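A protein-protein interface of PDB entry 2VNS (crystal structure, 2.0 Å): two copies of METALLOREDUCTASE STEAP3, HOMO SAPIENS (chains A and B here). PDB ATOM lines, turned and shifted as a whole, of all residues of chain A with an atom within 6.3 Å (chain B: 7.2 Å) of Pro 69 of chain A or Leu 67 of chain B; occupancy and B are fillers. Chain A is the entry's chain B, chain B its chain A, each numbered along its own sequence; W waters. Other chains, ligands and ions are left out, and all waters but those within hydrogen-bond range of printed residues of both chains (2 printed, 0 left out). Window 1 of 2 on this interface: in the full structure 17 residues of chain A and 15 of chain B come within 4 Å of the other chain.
Water W1 lies within hydrogen-bond range of OG of Ser 70 of chain B (2.7 Å), O of Ala 72 of chain A (2.9 Å) and O of Pro 69 of chain A (2.9 Å). Water W2 lies within hydrogen-bond range of OG of Ser 70 of chain A (2.7 Å), O of Pro 69 of chain B (2.8 Å) and O of Ala 65 of chain B (3.4 Å).
The backbone carbonyl oxygen (O) of Arg 41 of chain A sits at hydrogen-bond distance from the side-chain hydroxyl (OG1) of Thr 45 of chain A, 2.8 Å away. The side-chain carboxylate (OD1) of Asp 38 of chain B lies within salt-bridge range of the guanidinium group (NH2) of Arg 41 of chain B (3.2 Å). O of Arg 41 of chain B lies within hydrogen-bond range of OG1 of Thr 45 of chain B, at 2.8 Å.
Of the 15 printed residues of chain A, 9 touch a printed residue of chain B. Printed residues of chain A that touch a printed residue of chain B: Thr 45, Val 48, Gly 49, Ala 65, Leu 67, Phe 68, Pro 69, Ser 70 and Ala 71. Hydrophobic or aromatic side chains of chain A that line the printed part of chain B: Val 48, Pro 69 and Ala 71. Of the 14 printed residues of chain B, 7 touch a printed residue of chain A. Among the printed residues, no Asp or Glu carboxylate lies within 4 Å of a Lys or Arg side-chain nitrogen of the other chain.
Ala 65 of chain A touches Ser 70 of chain B, and with the chains exchanged Ser 70 of chain A touches Ala 65 of chain B. Leu 67 of chain A touches Pro 69 of chain B, and with the chains exchanged Pro 69 of chain A touches Leu 67 of chain B. Phe 68 of chain A touches Ser 70 of chain B, and with the chains exchanged Ser 70 of chain A touches Phe 68 of chain B. Ser 70 of chain A touches its own counterpart, Ser 70 of chain B. Positions printed for both chains: 41, 45, 65, 67, 68, 69, 70 and 74. Of the 20 pairs that touch across the chains among the printed residues, 12 have their exchanged pair printed and touching as well.
Among the printed residues, merely in contact across the chains: Phe 68 of chain A with Pro 69 of chain B (3.2 Å), Pro 69 of chain A with Phe 68 of chain B (3.3 Å), Pro 69 of chain A with Arg 66 of chain B (3.4 Å), Leu 67 of chain A with Pro 69 of chain B (3.4 Å), Thr 45 of chain A with Leu 67 of chain B (3.4 Å), Ser 70 of chain A with Ser 70 of chain B (3.5 Å), Pro 69 of chain A with Leu 67 of chain B (3.5 Å), Phe 68 of chain A with Phe 68 of chain B (3.6 Å), Thr 45 of chain A with Arg 41 of chain B (3.6 Å), Val 48 of chain A with Leu 67 of chain B (3.8 Å), Gly 49 of chain A with Leu 67 of chain B (3.8 Å), Ser 70 of chain A with Pro 69 of chain B (3.8 Å) and Pro 69 of chain A with Ser 70 of chain B (3.98 Å).
Of the printed residues of chain A, Leu 67 of chain B touches Thr 45 (3.4 Å), Val 48 (3.8 Å), Gly 49 (3.8 Å) and Pro 69 (3.5 Å). Printed residues of chain B within 4 Å of Thr 45 of chain A: Arg 41 (3.6 Å) and Leu 67 (3.4 Å). Of the printed residues of chain B, Ser 70 of chain A touches Ala 65 (2.9 Å), Arg 66 (3.3 Å), Phe 68 (2.9 Å), Pro 69 (3.8 Å) and Ser 70 (3.5 Å). Printed residues of chain A within 4 Å of Phe 68 of chain B: Phe 68, Pro 69 and Ser 70. Printed residues of chain B within 4 Å of Ala 65 of chain A: Ser 70 (2.8 Å). Ala 72 of chain A touches none of the printed residues of chain B. The nearest residue of chain A that does not touch Leu 67 of chain B is Ser 70 of chain A (4.6 Å). The nearest printed residue of chain B that does not touch Val 48 of chain A is Arg 63 of chain B (7.0 Å).
OG of Ser 70 of chain A is in hydrogen-bond range of O of Ala 65 of chain B (2.9 Å). O of Arg 66 of chain B is in hydrogen-bond range of N of Ser 70 of chain A, at 3.3 Å. NH2 of Arg 66 of chain B is in hydrogen-bond range of O of Val 48 of chain A, 3.0 Å away. N of Ser 70 of chain B lies within hydrogen-bond range of O of Phe 68 of chain A (2.9 Å). The side-chain hydroxyl (OG) of Ser 70 of chain B sits at hydrogen-bond distance from the backbone carbonyl oxygen (O) of Ala 65 of chain A (2.8 Å). The backbone carbonyl oxygen of Arg 66 of chain B lies within hydrogen-bond range of the backbone NH of Ala 71 of chain A, at 2.9 Å. N of Ser 70 of chain A lies within hydrogen-bond range of O of Phe 68 of chain B (2.9 Å).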
ATOM      1  N   ARG A  41      17.677 -25.703  20.185  1.00  0.00           N
ATOM      2  CA  ARG A  41      18.813 -25.719  21.073  1.00  0.00           C
ATOM      3  C   ARG A  41      19.916 -24.985  20.235  1.00  0.00           C
ATOM      4  O   ARG A  41      20.779 -24.255  20.769  1.00  0.00           O
ATOM      5  CB  ARG A  41      19.284 -27.149  21.380  1.00  0.00           C
ATOM      6  CG  ARG A  41      20.442 -27.203  22.326  1.00  0.00           C
ATOM      7  CD  ARG A  41      20.829 -28.632  22.724  1.00  0.00           C
ATOM      8  NE  ARG A  41      21.489 -29.312  21.597  1.00  0.00           N
ATOM      9  CZ  ARG A  41      20.971 -30.321  20.912  1.00  0.00           C
ATOM     10  NH1 ARG A  41      19.802 -30.831  21.262  1.00  0.00           N
ATOM     11  NH2 ARG A  41      21.632 -30.840  19.886  1.00  0.00           N
ATOM     12  N   ALA A  44      19.096 -21.235  20.181  1.00  0.00           N
ATOM     13  CA  ALA A  44      19.562 -20.699  21.461  1.00  0.00           C
ATOM     14  C   ALA A  44      21.085 -20.488  21.457  1.00  0.00           C
ATOM     15  O   ALA A  44      21.583 -19.470  21.933  1.00  0.00           O
ATOM     16  CB  ALA A  44      19.173 -21.636  22.612  1.00  0.00           C
ATOM     17  N   THR A  45      21.819 -21.462  20.934  1.00  0.00           N
ATOM     18  CA  THR A  45      23.294 -21.376  20.869  1.00  0.00           C
ATOM     19  C   THR A  45      23.704 -20.175  20.015  1.00  0.00           C
ATOM     20  O   THR A  45      24.516 -19.353  20.438  1.00  0.00           O
ATOM     21  CB  THR A  45      23.899 -22.693  20.342  1.00  0.00           C
ATOM     22  OG1 THR A  45      23.468 -23.776  21.180  1.00  0.00           O
ATOM     23  CG2 THR A  45      25.439 -22.668  20.331  1.00  0.00           C
ATOM     24  N   ARG A  46      23.082 -20.023  18.846  1.00  0.00           N
ATOM     25  CA  ARG A  46      23.408 -18.905  17.967  1.00  0.00           C
ATOM     26  C   ARG A  46      23.059 -17.531  18.574  1.00  0.00           C
ATOM     27  O   ARG A  46      23.850 -16.584  18.500  1.00  0.00           O
ATOM     28  CB  ARG A  46      22.721 -19.068  16.606  1.00  0.00           C
ATOM     29  CG  ARG A  46      23.250 -18.139  15.538  1.00  0.00           C
ATOM     30  CD  ARG A  46      24.733 -18.249  15.541  1.00  0.00           C
ATOM     31  NE  ARG A  46      25.390 -17.486  14.512  1.00  0.00           N
ATOM     32  CZ  ARG A  46      26.314 -17.969  13.695  1.00  0.00           C
ATOM     33  NH1 ARG A  46      26.699 -19.251  13.750  1.00  0.00           N
ATOM     34  NH2 ARG A  46      26.871 -17.148  12.812  1.00  0.00           N
ATOM     35  N   VAL A  48      22.645 -16.746  21.871  1.00  0.00           N
ATOM     36  CA  VAL A  48      23.553 -16.516  23.002  1.00  0.00           C
ATOM     37  C   VAL A  48      24.921 -16.058  22.478  1.00  0.00           C
ATOM     38  O   VAL A  48      25.514 -15.103  23.008  1.00  0.00           O
ATOM     39  CB  VAL A  48      23.761 -17.807  23.872  1.00  0.00           C
ATOM     40  CG1 VAL A  48      24.953 -17.636  24.816  1.00  0.00           C
ATOM     41  CG2 VAL A  48      22.498 -18.144  24.652  1.00  0.00           C
ATOM     42  N   GLY A  49      25.415 -16.733  21.439  1.00  0.00           N
ATOM     43  CA  GLY A  49      26.710 -16.370  20.836  1.00  0.00           C
ATOM     44  C   GLY A  49      26.705 -15.016  20.148  1.00  0.00           C
ATOM     45  O   GLY A  49      27.755 -14.412  19.924  1.00  0.00           O
ATOM     46  N   ALA A  65      17.002 -28.156  30.176  1.00  0.00           N
ATOM     47  CA  ALA A  65      18.077 -27.237  30.577  1.00  0.00           C
ATOM     48  C   ALA A  65      19.485 -27.851  30.500  1.00  0.00           C
ATOM     49  O   ALA A  65      20.444 -27.189  30.121  1.00  0.00           O
ATOM     50  CB  ALA A  65      17.820 -26.719  31.988  1.00  0.00           C
ATOM     51  N   LEU A  67      20.996 -29.840  28.536  1.00  0.00           N
ATOM     52  CA  LEU A  67      21.642 -29.840  27.201  1.00  0.00           C
ATOM     53  C   LEU A  67      21.796 -28.463  26.584  1.00  0.00           C
ATOM     54  O   LEU A  67      22.625 -28.294  25.695  1.00  0.00           O
ATOM     55  CB  LEU A  67      20.856 -30.704  26.211  1.00  0.00           C
ATOM     56  CG  LEU A  67      21.163 -32.203  26.197  1.00  0.00           C
ATOM     57  CD1 LEU A  67      21.178 -32.774  27.592  1.00  0.00           C
ATOM     58  CD2 LEU A  67      20.141 -32.934  25.321  1.00  0.00           C
ATOM     59  N   PHE A  68      20.978 -27.500  27.018  1.00  0.00           N
ATOM     60  CA  PHE A  68      20.997 -26.159  26.431  1.00  0.00           C
ATOM     61  C   PHE A  68      22.201 -25.349  26.904  1.00  0.00           C
ATOM     62  O   PHE A  68      22.753 -25.630  27.962  1.00  0.00           O
ATOM     63  CB  PHE A  68      19.695 -25.390  26.734  1.00  0.00           C
ATOM     64  CG  PHE A  68      18.618 -25.635  25.720  1.00  0.00           C
ATOM     65  CD1 PHE A  68      18.155 -26.923  25.483  1.00  0.00           C
ATOM     66  CD2 PHE A  68      18.109 -24.600  24.957  1.00  0.00           C
ATOM     67  CE1 PHE A  68      17.147 -27.157  24.523  1.00  0.00           C
ATOM     68  CE2 PHE A  68      17.104 -24.834  23.998  1.00  0.00           C
ATOM     69  CZ  PHE A  68      16.638 -26.095  23.780  1.00  0.00           C
ATOM     70  N   PRO A  69      22.617 -24.349  26.113  1.00  0.00           N
ATOM     71  CA  PRO A  69      23.715 -23.476  26.540  1.00  0.00           C
ATOM     72  C   PRO A  69      23.397 -22.846  27.885  1.00  0.00           C
ATOM     73  O   PRO A  69      22.258 -22.437  28.121  1.00  0.00           O
ATOM     74  CB  PRO A  69      23.776 -22.413  25.455  1.00  0.00           C
ATOM     75  CG  PRO A  69      22.588 -22.587  24.642  1.00  0.00           C
ATOM     76  CD  PRO A  69      22.119 -23.982  24.785  1.00  0.00           C
ATOM     77  N   SER A  70      24.387 -22.811  28.771  1.00  0.00           N
ATOM     78  CA  SER A  70      24.195 -22.309  30.134  1.00  0.00           C
ATOM     79  C   SER A  70      23.638 -20.898  30.162  1.00  0.00           C
ATOM     80  O   SER A  70      22.869 -20.559  31.046  1.00  0.00           O
ATOM     81  CB  SER A  70      25.490 -22.335  30.941  1.00  0.00           C
ATOM     82  OG  SER A  70      26.183 -23.532  30.693  1.00  0.00           O
ATOM     83  N   ALA A  71      24.037 -20.075  29.200  1.00  0.00           N
ATOM     84  CA  ALA A  71      23.587 -18.678  29.150  1.00  0.00           C
ATOM     85  C   ALA A  71      22.092 -18.526  28.826  1.00  0.00           C
ATOM     86  O   ALA A  71      21.512 -17.446  29.046  1.00  0.00           O
ATOM     87  CB  ALA A  71      24.415 -17.903  28.159  1.00  0.00           C
ATOM     88  N   ALA A  72      21.465 -19.562  28.277  1.00  0.00           N
ATOM     89  CA  ALA A  72      20.018 -19.539  28.036  1.00  0.00           C
ATOM     90  C   ALA A  72      19.264 -19.954  29.315  1.00  0.00           C
ATOM     91  O   ALA A  72      19.676 -20.884  30.041  1.00  0.00           O
ATOM     92  CB  ALA A  72      19.650 -20.442  26.859  1.00  0.00           C
ATOM     93  N   GLN A  73      18.195 -19.229  29.629  1.00  0.00           N
ATOM     94  CA  GLN A  73      17.340 -19.576  30.759  1.00  0.00           C
ATOM     95  C   GLN A  73      16.192 -20.451  30.303  1.00  0.00           C
ATOM     96  O   GLN A  73      15.279 -19.980  29.643  1.00  0.00           O
ATOM     97  CB  GLN A  73      16.769 -18.324  31.398  1.00  0.00           C
ATOM     98  CG  GLN A  73      17.742 -17.677  32.312  1.00  0.00           C
ATOM     99  CD  GLN A  73      17.586 -16.213  32.297  1.00  0.00           C
ATOM    100  OE1 GLN A  73      17.728 -15.576  31.221  1.00  0.00           O
ATOM    101  NE2 GLN A  73      17.280 -15.632  33.463  1.00  0.00           N
ATOM    102  N   VAL A  74      16.254 -21.728  30.661  1.00  0.00           N
ATOM    103  CA  VAL A  74      15.248 -22.690  30.264  1.00  0.00           C
ATOM    104  C   VAL A  74      14.259 -22.778  31.417  1.00  0.00           C
ATOM    105  O   VAL A  74      14.649 -22.967  32.571  1.00  0.00           O
ATOM    106  CB  VAL A  74      15.840 -24.088  29.955  1.00  0.00           C
ATOM    107  CG1 VAL A  74      14.719 -25.094  29.630  1.00  0.00           C
ATOM    108  CG2 VAL A  74      16.884 -24.004  28.809  1.00  0.00           C
ATOM    109  N   SER B  36      37.328 -26.004  23.747  1.00  0.00           N
ATOM    110  CA  SER B  36      36.349 -24.940  23.976  1.00  0.00           C
ATOM    111  C   SER B  36      35.513 -24.861  22.698  1.00  0.00           C
ATOM    112  O   SER B  36      34.528 -24.126  22.636  1.00  0.00           O
ATOM    113  CB  SER B  36      36.982 -23.590  24.248  1.00  0.00           C
ATOM    114  OG  SER B  36      37.443 -23.524  25.574  1.00  0.00           O
ATOM    115  N   ASP B  38      33.728 -26.178  18.728  1.00  0.00           N
ATOM    116  CA  ASP B  38      32.502 -26.841  18.273  1.00  0.00           C
ATOM    117  C   ASP B  38      32.520 -28.323  18.588  1.00  0.00           C
ATOM    118  O   ASP B  38      31.520 -28.893  19.018  1.00  0.00           O
ATOM    119  CB  ASP B  38      32.301 -26.658  16.779  1.00  0.00           C
ATOM    120  CG  ASP B  38      31.877 -25.251  16.408  1.00  0.00           C
ATOM    121  OD1 ASP B  38      31.234 -24.549  17.216  1.00  0.00           O
ATOM    122  OD2 ASP B  38      32.209 -24.855  15.288  1.00  0.00           O
ATOM    123  N   ARG B  41      32.167 -29.051  22.278  1.00  0.00           N
ATOM    124  CA  ARG B  41      30.938 -28.541  22.858  1.00  0.00           C
ATOM    125  C   ARG B  41      29.933 -29.671  22.494  1.00  0.00           C
ATOM    126  O   ARG B  41      29.057 -30.060  23.274  1.00  0.00           O
ATOM    127  CB  ARG B  41      30.541 -27.250  22.158  1.00  0.00           C
ATOM    128  CG  ARG B  41      29.269 -26.640  22.673  1.00  0.00           C
ATOM    129  CD  ARG B  41      29.182 -25.207  22.263  1.00  0.00           C
ATOM    130  NE  ARG B  41      29.277 -25.063  20.811  1.00  0.00           N
ATOM    131  CZ  ARG B  41      28.308 -25.392  19.987  1.00  0.00           C
ATOM    132  NH1 ARG B  41      27.192 -25.855  20.491  1.00  0.00           N
ATOM    133  NH2 ARG B  41      28.451 -25.256  18.676  1.00  0.00           N
ATOM    134  N   THR B  45      27.850 -32.298  24.896  1.00  0.00           N
ATOM    135  CA  THR B  45      26.399 -32.424  24.750  1.00  0.00           C
ATOM    136  C   THR B  45      26.033 -33.902  24.635  1.00  0.00           C
ATOM    137  O   THR B  45      25.103 -34.362  25.288  1.00  0.00           O
ATOM    138  CB  THR B  45      25.909 -31.655  23.526  1.00  0.00           C
ATOM    139  OG1 THR B  45      26.298 -30.273  23.643  1.00  0.00           O
ATOM    140  CG2 THR B  45      24.390 -31.767  23.366  1.00  0.00           C
ATOM    141  N   LYS B  62      34.784 -18.608  31.713  1.00  0.00           N
ATOM    142  CA  LYS B  62      33.637 -17.715  31.879  1.00  0.00           C
ATOM    143  C   LYS B  62      32.892 -17.592  30.561  1.00  0.00           C
ATOM    144  O   LYS B  62      31.685 -17.832  30.496  1.00  0.00           O
ATOM    145  CB  LYS B  62      34.070 -16.341  32.382  1.00  0.00           C
ATOM    146  CG  LYS B  62      32.896 -15.478  32.770  1.00  0.00           C
ATOM    147  CD  LYS B  62      33.320 -14.154  33.377  1.00  0.00           C
ATOM    148  CE  LYS B  62      32.116 -13.204  33.430  1.00  0.00           C
ATOM    149  NZ  LYS B  62      32.502 -11.790  33.785  1.00  0.00           N
ATOM    150  N   ARG B  63      33.636 -17.262  29.511  1.00  0.00           N
ATOM    151  CA  ARG B  63      33.074 -17.085  28.175  1.00  0.00           C
ATOM    152  C   ARG B  63      32.618 -18.431  27.583  1.00  0.00           C
ATOM    153  O   ARG B  63      31.542 -18.539  26.999  1.00  0.00           O
ATOM    154  CB  ARG B  63      34.086 -16.411  27.247  1.00  0.00           C
ATOM    155  N   THR B  64      33.446 -19.454  27.749  1.00  0.00           N
ATOM    156  CA  THR B  64      33.170 -20.776  27.174  1.00  0.00           C
ATOM    157  C   THR B  64      31.907 -21.397  27.794  1.00  0.00           C
ATOM    158  O   THR B  64      31.074 -21.960  27.093  1.00  0.00           O
ATOM    159  CB  THR B  64      34.386 -21.715  27.375  1.00  0.00           C
ATOM    160  OG1 THR B  64      35.537 -21.159  26.716  1.00  0.00           O
ATOM    161  CG2 THR B  64      34.102 -23.151  26.838  1.00  0.00           C
ATOM    162  N   ALA B  65      31.768 -21.261  29.106  1.00  0.00           N
ATOM    163  CA  ALA B  65      30.635 -21.845  29.834  1.00  0.00           C
ATOM    164  C   ALA B  65      29.270 -21.427  29.256  1.00  0.00           C
ATOM    165  O   ALA B  65      28.348 -22.242  29.165  1.00  0.00           O
ATOM    166  CB  ALA B  65      30.721 -21.504  31.328  1.00  0.00           C
ATOM    167  N   ARG B  66      29.161 -20.168  28.839  1.00  0.00           N
ATOM    168  CA  ARG B  66      27.892 -19.592  28.340  1.00  0.00           C
ATOM    169  C   ARG B  66      27.254 -20.406  27.202  1.00  0.00           C
ATOM    170  O   ARG B  66      26.040 -20.503  27.116  1.00  0.00           O
ATOM    171  CB  ARG B  66      28.106 -18.149  27.860  1.00  0.00           C
ATOM    172  CG  ARG B  66      28.748 -17.239  28.906  1.00  0.00           C
ATOM    173  CD  ARG B  66      28.382 -15.762  28.763  1.00  0.00           C
ATOM    174  NE  ARG B  66      28.185 -15.377  27.371  1.00  0.00           N
ATOM    175  CZ  ARG B  66      27.036 -14.959  26.848  1.00  0.00           C
ATOM    176  NH1 ARG B  66      25.950 -14.819  27.598  1.00  0.00           N
ATOM    177  NH2 ARG B  66      26.977 -14.666  25.556  1.00  0.00           N
ATOM    178  N   LEU B  67      28.076 -20.961  26.320  1.00  0.00           N
ATOM    179  CA  LEU B  67      27.585 -21.746  25.169  1.00  0.00           C
ATOM    180  C   LEU B  67      27.489 -23.260  25.412  1.00  0.00           C
ATOM    181  O   LEU B  67      26.855 -23.965  24.642  1.00  0.00           O
ATOM    182  CB  LEU B  67      28.485 -21.512  23.950  1.00  0.00           C
ATOM    183  CG  LEU B  67      28.397 -20.131  23.291  1.00  0.00           C
ATOM    184  CD1 LEU B  67      29.481 -19.939  22.236  1.00  0.00           C
ATOM    185  CD2 LEU B  67      27.046 -19.971  22.684  1.00  0.00           C
ATOM    186  N   PHE B  68      28.171 -23.764  26.433  1.00  0.00           N
ATOM    187  CA  PHE B  68      28.186 -25.209  26.699  1.00  0.00           C
ATOM    188  C   PHE B  68      26.901 -25.656  27.395  1.00  0.00           C
ATOM    189  O   PHE B  68      26.253 -24.858  28.063  1.00  0.00           O
ATOM    190  CB  PHE B  68      29.412 -25.626  27.536  1.00  0.00           C
ATOM    191  CG  PHE B  68      30.618 -26.008  26.704  1.00  0.00           C
ATOM    192  CD1 PHE B  68      31.180 -25.105  25.822  1.00  0.00           C
ATOM    193  CD2 PHE B  68      31.175 -27.285  26.787  1.00  0.00           C
ATOM    194  CE1 PHE B  68      32.288 -25.449  25.042  1.00  0.00           C
ATOM    195  CE2 PHE B  68      32.317 -27.645  26.014  1.00  0.00           C
ATOM    196  CZ  PHE B  68      32.854 -26.736  25.136  1.00  0.00           C
ATOM    197  N   PRO B  69      26.539 -26.946  27.242  1.00  0.00           N
ATOM    198  CA  PRO B  69      25.372 -27.460  27.951  1.00  0.00           C
ATOM    199  C   PRO B  69      25.506 -27.187  29.433  1.00  0.00           C
ATOM    200  O   PRO B  69      26.617 -27.285  29.976  1.00  0.00           O
ATOM    201  CB  PRO B  69      25.376 -28.970  27.638  1.00  0.00           C
ATOM    202  CG  PRO B  69      26.673 -29.259  26.988  1.00  0.00           C
ATOM    203  CD  PRO B  69      27.180 -27.974  26.411  1.00  0.00           C
ATOM    204  N   SER B  70      24.397 -26.795  30.054  1.00  0.00           N
ATOM    205  CA  SER B  70      24.349 -26.433  31.470  1.00  0.00           C
ATOM    206  C   SER B  70      24.841 -27.513  32.387  1.00  0.00           C
ATOM    207  O   SER B  70      25.419 -27.201  33.411  1.00  0.00           O
ATOM    208  CB  SER B  70      22.915 -26.106  31.891  1.00  0.00           C
ATOM    209  OG  SER B  70      22.322 -25.263  30.922  1.00  0.00           O
ATOM    210  N   VAL B  74      32.220 -26.283  33.353  1.00  0.00           N
ATOM    211  CA  VAL B  74      33.307 -25.697  32.580  1.00  0.00           C
ATOM    212  C   VAL B  74      34.181 -24.911  33.532  1.00  0.00           C
ATOM    213  O   VAL B  74      33.693 -24.106  34.320  1.00  0.00           O
ATOM    214  CB  VAL B  74      32.782 -24.777  31.483  1.00  0.00           C
ATOM    215  CG1 VAL B  74      33.958 -24.163  30.670  1.00  0.00           C
ATOM    216  CG2 VAL B  74      31.799 -25.557  30.590  1.00  0.00           C
HETATM  217  O   HOH W   1      20.414 -23.660  29.965  1.00  0.00           O
HETATM  218  O   HOH W   2      28.297 -25.184  30.899  1.00  0.00           O
